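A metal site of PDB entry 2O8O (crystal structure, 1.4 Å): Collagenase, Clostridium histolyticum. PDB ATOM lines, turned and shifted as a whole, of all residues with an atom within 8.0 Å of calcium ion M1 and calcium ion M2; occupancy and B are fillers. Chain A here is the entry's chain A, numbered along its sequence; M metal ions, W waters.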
ATOM      1  N   GLU A  13       7.926   8.236  11.143  1.00  0.00           N
ATOM      2  CA  GLU A  13       7.722   7.554  12.409  1.00  0.00           C
ATOM      3  C   GLU A  13       8.727   8.065  13.403  1.00  0.00           C
ATOM      4  O   GLU A  13       9.742   8.678  13.081  1.00  0.00           O
ATOM      5  CB  GLU A  13       7.913   6.032  12.269  1.00  0.00           C
ATOM      6  CG  GLU A  13       9.292   5.677  11.767  1.00  0.00           C
ATOM      7  CD  GLU A  13       9.565   4.187  11.798  1.00  0.00           C
ATOM      8  OE1 GLU A  13       9.146   3.570  12.798  1.00  0.00           O
ATOM      9  OE2 GLU A  13      10.386   3.759  10.960  1.00  0.00           O
ATOM     10  N   LYS A  14       8.641   7.857  14.651  1.00  0.00           N
ATOM     11  CA  LYS A  14       9.319   8.241  15.862  1.00  0.00           C
ATOM     12  C   LYS A  14       9.617   6.990  16.694  1.00  0.00           C
ATOM     13  O   LYS A  14       8.839   6.435  17.451  1.00  0.00           O
ATOM     14  CB  LYS A  14       8.546   9.285  16.683  1.00  0.00           C
ATOM     15  CG  LYS A  14       8.312  10.741  16.418  1.00  0.00           C
ATOM     16  CD  LYS A  14       8.287  11.260  14.998  1.00  0.00           C
ATOM     17  CE  LYS A  14       9.250  12.414  14.722  1.00  0.00           C
ATOM     18  NZ  LYS A  14      10.005  12.168  13.454  1.00  0.00           N
ATOM     19  N   GLU A  15      10.861   6.506  16.535  1.00  0.00           N
ATOM     20  CA  GLU A  15      11.316   5.395  17.370  1.00  0.00           C
ATOM     21  C   GLU A  15      11.687   5.927  18.743  1.00  0.00           C
ATOM     22  O   GLU A  15      12.073   7.118  18.869  1.00  0.00           O
ATOM     23  CB  GLU A  15      12.536   4.666  16.836  1.00  0.00           C
ATOM     24  CG  GLU A  15      12.304   3.929  15.516  1.00  0.00           C
ATOM     25  CD  GLU A  15      11.510   2.636  15.649  1.00  0.00           C
ATOM     26  OE1 GLU A  15      11.335   2.122  16.773  1.00  0.00           O
ATOM     27  OE2 GLU A  15      11.149   2.093  14.584  1.00  0.00           O
ATOM     28  N   ASN A  16      11.584   5.076  19.727  1.00  0.00           N
ATOM     29  CA  ASN A  16      11.101   3.699  19.750  1.00  0.00           C
ATOM     30  C   ASN A  16       9.576   3.664  19.782  1.00  0.00           C
ATOM     31  O   ASN A  16       8.985   4.320  20.636  1.00  0.00           O
ATOM     32  CB  ASN A  16      11.692   3.040  20.993  1.00  0.00           C
ATOM     33  CG  ASN A  16      11.344   1.605  21.211  1.00  0.00           C
ATOM     34  OD1 ASN A  16      10.198   1.218  21.042  1.00  0.00           O
ATOM     35  ND2 ASN A  16      12.296   0.762  21.592  1.00  0.00           N
ATOM     36  N   ASN A  17       9.028   2.908  18.858  1.00  0.00           N
ATOM     37  CA  ASN A  17       7.601   2.743  18.729  1.00  0.00           C
ATOM     38  C   ASN A  17       7.205   1.271  18.683  1.00  0.00           C
ATOM     39  O   ASN A  17       6.272   0.851  18.034  1.00  0.00           O
ATOM     40  CB  ASN A  17       7.050   3.438  17.484  1.00  0.00           C
ATOM     41  CG  ASN A  17       7.731   2.966  16.216  1.00  0.00           C
ATOM     42  OD1 ASN A  17       8.419   1.939  16.250  1.00  0.00           O
ATOM     43  ND2 ASN A  17       7.562   3.725  15.147  1.00  0.00           N
ATOM     44  N   ASP A  18       7.889   0.475  19.488  1.00  0.00           N
ATOM     45  CA  ASP A  18       7.721  -0.989  19.425  1.00  0.00           C
ATOM     46  C   ASP A  18       6.570  -1.562  20.255  1.00  0.00           C
ATOM     47  O   ASP A  18       6.336  -2.767  20.256  1.00  0.00           O
ATOM     48  CB  ASP A  18       9.067  -1.609  19.803  1.00  0.00           C
ATOM     49  CG  ASP A  18      10.202  -1.326  18.821  1.00  0.00           C
ATOM     50  OD1 ASP A  18      11.325  -1.798  19.106  1.00  0.00           O
ATOM     51  OD2 ASP A  18      10.080  -0.644  17.777  1.00  0.00           O
ATOM     52  N   SER A  19       5.833  -0.727  20.960  1.00  0.00           N
ATOM     53  CA  SER A  19       4.689  -1.134  21.768  1.00  0.00           C
ATOM     54  C   SER A  19       3.613  -0.074  21.620  1.00  0.00           C
ATOM     55  O   SER A  19       3.946   1.017  21.239  1.00  0.00           O
ATOM     56  CB  SER A  19       5.137  -1.333  23.206  1.00  0.00           C
ATOM     57  OG  SER A  19       5.581  -0.081  23.717  1.00  0.00           O
ATOM     58  N   LYS A  22       3.931   3.331  23.075  1.00  0.00           N
ATOM     59  CA  LYS A  22       4.880   4.205  22.415  1.00  0.00           C
ATOM     60  C   LYS A  22       4.551   4.420  20.946  1.00  0.00           C
ATOM     61  O   LYS A  22       5.390   4.802  20.123  1.00  0.00           O
ATOM     62  CB  LYS A  22       6.263   3.555  22.491  1.00  0.00           C
ATOM     63  CG  LYS A  22       6.709   3.312  23.945  1.00  0.00           C
ATOM     64  CD  LYS A  22       7.983   2.511  23.988  1.00  0.00           C
ATOM     65  CE  LYS A  22       7.976   1.231  23.178  1.00  0.00           C
ATOM     66  NZ  LYS A  22       8.529   0.001  23.750  1.00  0.00           N
ATOM     67  N   THR A  24       3.459   5.766  17.375  1.00  0.00           N
ATOM     68  CA  THR A  24       3.566   7.000  16.660  1.00  0.00           C
ATOM     69  C   THR A  24       2.172   7.435  16.216  1.00  0.00           C
ATOM     70  O   THR A  24       1.452   6.696  15.525  1.00  0.00           O
ATOM     71  CB  THR A  24       4.418   6.858  15.387  1.00  0.00           C
ATOM     72  OG1 THR A  24       5.681   6.391  15.837  1.00  0.00           O
ATOM     73  CG2 THR A  24       4.516   8.168  14.629  1.00  0.00           C
ATOM     74  N   GLN A  34       6.317   7.994   6.624  1.00  0.00           N
ATOM     75  CA  GLN A  34       7.497   7.248   6.206  1.00  0.00           C
ATOM     76  C   GLN A  34       8.062   6.404   7.349  1.00  0.00           C
ATOM     77  O   GLN A  34       8.181   6.919   8.451  1.00  0.00           O
ATOM     78  CB  GLN A  34       8.578   8.224   5.735  1.00  0.00           C
ATOM     79  CG  GLN A  34       8.142   8.984   4.478  1.00  0.00           C
ATOM     80  CD  GLN A  34       9.333   9.583   3.749  1.00  0.00           C
ATOM     81  OE1 GLN A  34       9.350   9.723   2.511  1.00  0.00           O
ATOM     82  NE2 GLN A  34      10.341   9.926   4.532  1.00  0.00           N
ATOM     83  N   GLY A  35       8.391   5.146   7.089  1.00  0.00           N
ATOM     84  CA  GLY A  35       9.038   4.354   8.115  1.00  0.00           C
ATOM     85  C   GLY A  35       9.969   3.321   7.481  1.00  0.00           C
ATOM     86  O   GLY A  35      10.058   3.149   6.266  1.00  0.00           O
ATOM     87  N   SER A  36      10.642   2.642   8.400  1.00  0.00           N
ATOM     88  CA  SER A  36      11.541   1.570   8.019  1.00  0.00           C
ATOM     89  C   SER A  36      11.523   0.454   9.063  1.00  0.00           C
ATOM     90  O   SER A  36      11.284   0.761  10.227  1.00  0.00           O
ATOM     91  CB  SER A  36      12.965   2.105   7.814  1.00  0.00           C
ATOM     92  OG  SER A  36      13.597   2.401   9.037  1.00  0.00           O
ATOM     93  N   LEU A  37      11.773  -0.768   8.615  1.00  0.00           N
ATOM     94  CA  LEU A  37      11.901  -1.949   9.441  1.00  0.00           C
ATOM     95  C   LEU A  37      13.171  -2.686   8.999  1.00  0.00           C
ATOM     96  O   LEU A  37      13.148  -3.704   8.326  1.00  0.00           O
ATOM     97  CB  LEU A  37      10.705  -2.888   9.326  1.00  0.00           C
ATOM     98  CG  LEU A  37       9.383  -2.326   9.895  1.00  0.00           C
ATOM     99  CD1 LEU A  37       8.201  -3.161   9.463  1.00  0.00           C
ATOM    100  CD2 LEU A  37       9.388  -2.235  11.407  1.00  0.00           C
ATOM    101  N   LEU A  38      14.287  -2.090   9.383  1.00  0.00           N
ATOM    102  CA  LEU A  38      15.634  -2.562   9.041  1.00  0.00           C
ATOM    103  C   LEU A  38      16.229  -3.361  10.193  1.00  0.00           C
ATOM    104  O   LEU A  38      16.171  -2.913  11.325  1.00  0.00           O
ATOM    105  CB  LEU A  38      16.565  -1.395   8.696  1.00  0.00           C
ATOM    106  CG  LEU A  38      15.949  -0.338   7.773  1.00  0.00           C
ATOM    107  CD1 LEU A  38      16.897   0.865   7.712  1.00  0.00           C
ATOM    108  CD2 LEU A  38      15.649  -0.872   6.385  1.00  0.00           C
ATOM    109  N   ASP A  40      16.943  -5.477  13.273  1.00  0.00           N
ATOM    110  CA  ASP A  40      16.163  -5.929  14.416  1.00  0.00           C
ATOM    111  C   ASP A  40      15.040  -4.955  14.778  1.00  0.00           C
ATOM    112  O   ASP A  40      14.358  -5.183  15.789  1.00  0.00           O
ATOM    113  CB  ASP A  40      17.046  -6.247  15.611  1.00  0.00           C
ATOM    114  CG  ASP A  40      17.766  -5.091  16.239  1.00  0.00           C
ATOM    115  OD1 ASP A  40      17.412  -3.932  16.018  1.00  0.00           O
ATOM    116  OD2 ASP A  40      18.748  -5.433  16.961  1.00  0.00           O
ATOM    117  N   ASP A  41      14.812  -3.916  13.987  1.00  0.00           N
ATOM    118  CA  ASP A  41      13.578  -3.155  14.136  1.00  0.00           C
ATOM    119  C   ASP A  41      12.504  -3.886  13.336  1.00  0.00           C
ATOM    120  O   ASP A  41      12.474  -3.744  12.100  1.00  0.00           O
ATOM    121  CB  ASP A  41      13.755  -1.725  13.667  1.00  0.00           C
ATOM    122  CG  ASP A  41      12.549  -0.856  13.780  1.00  0.00           C
ATOM    123  OD1 ASP A  41      11.835  -1.006  14.796  1.00  0.00           O
ATOM    124  OD2 ASP A  41      12.296  -0.032  12.875  1.00  0.00           O
ATOM    125  N   SER A  42      11.666  -4.667  14.042  1.00  0.00           N
ATOM    126  CA  SER A  42      10.707  -5.510  13.333  1.00  0.00           C
ATOM    127  C   SER A  42       9.252  -5.082  13.498  1.00  0.00           C
ATOM    128  O   SER A  42       8.404  -5.724  12.857  1.00  0.00           O
ATOM    129  CB  SER A  42      10.738  -6.971  13.783  1.00  0.00           C
ATOM    130  OG  SER A  42      10.890  -7.068  15.144  1.00  0.00           O
ATOM    131  N   ARG A  43       9.015  -4.090  14.320  1.00  0.00           N
ATOM    132  CA  ARG A  43       7.687  -3.601  14.665  1.00  0.00           C
ATOM    133  C   ARG A  43       7.653  -2.090  14.757  1.00  0.00           C
ATOM    134  O   ARG A  43       8.527  -1.532  15.447  1.00  0.00           O
ATOM    135  CB  ARG A  43       7.236  -4.142  16.073  1.00  0.00           C
ATOM    136  CG  ARG A  43       7.258  -5.638  16.171  1.00  0.00           C
ATOM    137  CD  ARG A  43       7.234  -6.057  17.609  1.00  0.00           C
ATOM    138  NE  ARG A  43       6.146  -5.567  18.403  1.00  0.00           N
ATOM    139  CZ  ARG A  43       5.010  -6.223  18.637  1.00  0.00           C
ATOM    140  NH1 ARG A  43       4.720  -7.422  18.116  1.00  0.00           N
ATOM    141  NH2 ARG A  43       4.157  -5.584  19.417  1.00  0.00           N
ATOM    142  N   ASP A  44       6.666  -1.464  14.127  1.00  0.00           N
ATOM    143  CA  ASP A  44       6.383  -0.042  14.263  1.00  0.00           C
ATOM    144  C   ASP A  44       4.894   0.113  14.570  1.00  0.00           C
ATOM    145  O   ASP A  44       4.055  -0.201  13.726  1.00  0.00           O
ATOM    146  CB  ASP A  44       6.729   0.688  12.979  1.00  0.00           C
ATOM    147  CG  ASP A  44       8.184   0.735  12.610  1.00  0.00           C
ATOM    148  OD1 ASP A  44       9.031   0.519  13.498  1.00  0.00           O
ATOM    149  OD2 ASP A  44       8.503   0.988  11.422  1.00  0.00           O
ATOM    150  N   TYR A  45       4.609   0.548  15.789  1.00  0.00           N
ATOM    151  CA  TYR A  45       3.238   0.820  16.201  1.00  0.00           C
ATOM    152  C   TYR A  45       2.834   2.245  15.877  1.00  0.00           C
ATOM    153  O   TYR A  45       3.618   3.179  16.147  1.00  0.00           O
ATOM    154  CB  TYR A  45       3.024   0.585  17.696  1.00  0.00           C
ATOM    155  CG  TYR A  45       2.046  -0.534  18.003  1.00  0.00           C
ATOM    156  CD1 TYR A  45       2.405  -1.648  18.731  1.00  0.00           C
ATOM    157  CD2 TYR A  45       0.744  -0.507  17.552  1.00  0.00           C
ATOM    158  CE1 TYR A  45       1.591  -2.705  19.048  1.00  0.00           C
ATOM    159  CE2 TYR A  45      -0.101  -1.568  17.852  1.00  0.00           C
ATOM    160  CZ  TYR A  45       0.302  -2.655  18.590  1.00  0.00           C
ATOM    161  OH  TYR A  45      -0.598  -3.663  18.849  1.00  0.00           O
ATOM    162  N   TYR A  46       1.632   2.383  15.343  1.00  0.00           N
ATOM    163  CA  TYR A  46       0.988   3.667  15.105  1.00  0.00           C
ATOM    164  C   TYR A  46      -0.387   3.700  15.772  1.00  0.00           C
ATOM    165  O   TYR A  46      -0.939   2.654  16.113  1.00  0.00           O
ATOM    166  CB  TYR A  46       0.805   3.909  13.611  1.00  0.00           C
ATOM    167  CG  TYR A  46       2.061   3.938  12.818  1.00  0.00           C
ATOM    168  CD1 TYR A  46       2.658   2.795  12.332  1.00  0.00           C
ATOM    169  CD2 TYR A  46       2.678   5.137  12.549  1.00  0.00           C
ATOM    170  CE1 TYR A  46       3.827   2.837  11.586  1.00  0.00           C
ATOM    171  CE2 TYR A  46       3.832   5.225  11.814  1.00  0.00           C
ATOM    172  CZ  TYR A  46       4.405   4.068  11.346  1.00  0.00           C
ATOM    173  OH  TYR A  46       5.578   4.196  10.614  1.00  0.00           O
ATOM    174  N   LEU A 106      -0.336  -1.908  14.015  1.00  0.00           N
ATOM    175  CA  LEU A 106       0.967  -2.486  14.177  1.00  0.00           C
ATOM    176  C   LEU A 106       1.468  -2.867  12.765  1.00  0.00           C
ATOM    177  O   LEU A 106       0.866  -3.753  12.141  1.00  0.00           O
ATOM    178  CB  LEU A 106       0.958  -3.721  15.069  1.00  0.00           C
ATOM    179  CG  LEU A 106       2.276  -4.507  15.104  1.00  0.00           C
ATOM    180  CD1 LEU A 106       3.360  -3.656  15.709  1.00  0.00           C
ATOM    181  CD2 LEU A 106       2.036  -5.787  15.890  1.00  0.00           C
ATOM    182  N   VAL A 107       2.525  -2.224  12.346  1.00  0.00           N
ATOM    183  CA  VAL A 107       3.239  -2.589  11.102  1.00  0.00           C
ATOM    184  C   VAL A 107       4.406  -3.469  11.512  1.00  0.00           C
ATOM    185  O   VAL A 107       5.203  -3.103  12.393  1.00  0.00           O
ATOM    186  CB  VAL A 107       3.699  -1.348  10.324  1.00  0.00           C
ATOM    187  CG1 VAL A 107       4.514  -1.768   9.119  1.00  0.00           C
ATOM    188  CG2 VAL A 107       2.518  -0.462   9.934  1.00  0.00           C
ATOM    189  N   GLY A 114      13.307  -3.523   5.074  1.00  0.00           N
ATOM    190  CA  GLY A 114      13.035  -2.508   4.074  1.00  0.00           C
ATOM    191  C   GLY A 114      12.356  -1.276   4.639  1.00  0.00           C
ATOM    192  O   GLY A 114      12.006  -1.210   5.827  1.00  0.00           O
ATOM    193  N   TYR A 116       9.139   1.652   3.940  1.00  0.00           N
ATOM    194  CA  TYR A 116       7.753   1.670   3.529  1.00  0.00           C
ATOM    195  C   TYR A 116       7.165   3.074   3.700  1.00  0.00           C
ATOM    196  O   TYR A 116       7.678   3.946   4.418  1.00  0.00           O
ATOM    197  CB  TYR A 116       6.911   0.611   4.305  1.00  0.00           C
ATOM    198  CG  TYR A 116       6.822   0.916   5.789  1.00  0.00           C
ATOM    199  CD1 TYR A 116       5.830   1.680   6.341  1.00  0.00           C
ATOM    200  CD2 TYR A 116       7.773   0.440   6.678  1.00  0.00           C
ATOM    201  CE1 TYR A 116       5.728   1.985   7.665  1.00  0.00           C
ATOM    202  CE2 TYR A 116       7.711   0.745   8.021  1.00  0.00           C
ATOM    203  CZ  TYR A 116       6.682   1.511   8.508  1.00  0.00           C
ATOM    204  OH  TYR A 116       6.610   1.806   9.830  1.00  0.00           O
HETATM  205 CA    CA M   1      10.824   1.759  12.294  1.00  0.00          CA
HETATM  206 CA    CA M   2       9.974   0.293  15.650  1.00  0.00          CA
HETATM  207  O   HOH W   1      12.941   2.919  12.033  1.00  0.00           O
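The side-chain amide nitrogen (ND2) of Asn 17 lies close to the side-chain carboxylate (OE1) of Glu 13.
The backbone carbonyl oxygen (O) of Asn 17 lies within hydrogen-bond range of the backbone NH (N) of Tyr 45.
N of Asp 44 lies within hydrogen-bond range of O of Val 107 (2.8 Å).
The side-chain hydroxyl (OH) of Tyr 116 lies close to the side-chain carboxylate (OD2) of Asp 44 (2.6 Å).
The backbone NH (N) of Asp 18 sits at hydrogen-bond distance from the side-chain amide oxygen (OD1) of Asn 16 (2.9 Å).
The backbone NH of Glu 13 is in hydrogen-bond range of the backbone carbonyl oxygen of Gln 34 (3.0 Å).
The side-chain hydroxyl (OG1) of Thr 24 sits at hydrogen-bond distance from the side-chain amide nitrogen (ND2) of Asn 17, 3.3 Å away.
Five residues have an atom within 4 Å of calcium ion M1: Glu 13, Glu 15, Ser 36, Asp 41 and Asp 44.
The nearest printed residue that does not touch calcium ion M2 is Glu 13 (4.4 Å).
OE2 of Glu 15 binds calcium ion M1.
O of Ser 36 is bound to calcium ion M1 (2.3 Å).
Calcium ion M1 is bound by the side-chain carboxylate (OD2) of Asp 41 (2.4 Å).
Water W1 is bound to calcium ion M1 (2.4 Å).
Calcium ion M1 is bound by the side-chain carboxylate (OE2) of Glu 13, at 2.4 Å.
Calcium ion M1 is bound by the side-chain carboxylate (OD1) of Asp 44, 2.5 Å away.
OE1 of Glu 13 is bound to calcium ion M1 (2.5 Å).
Calcium ion M1 is bound by OD2 of Asp 44, 2.6 Å away.
Calcium ion M1 has eight donor atoms within binding distance.
Calcium ion M2 is bound by OD2 of Asp 18, O of Arg 43, OD1 of Asn 17, OD1 of Asp 44, OE2 of Glu 15, OD1 of Asp 41 and OE1 of Glu 15.
Calcium ion M2 has seven donor atoms within binding distance.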
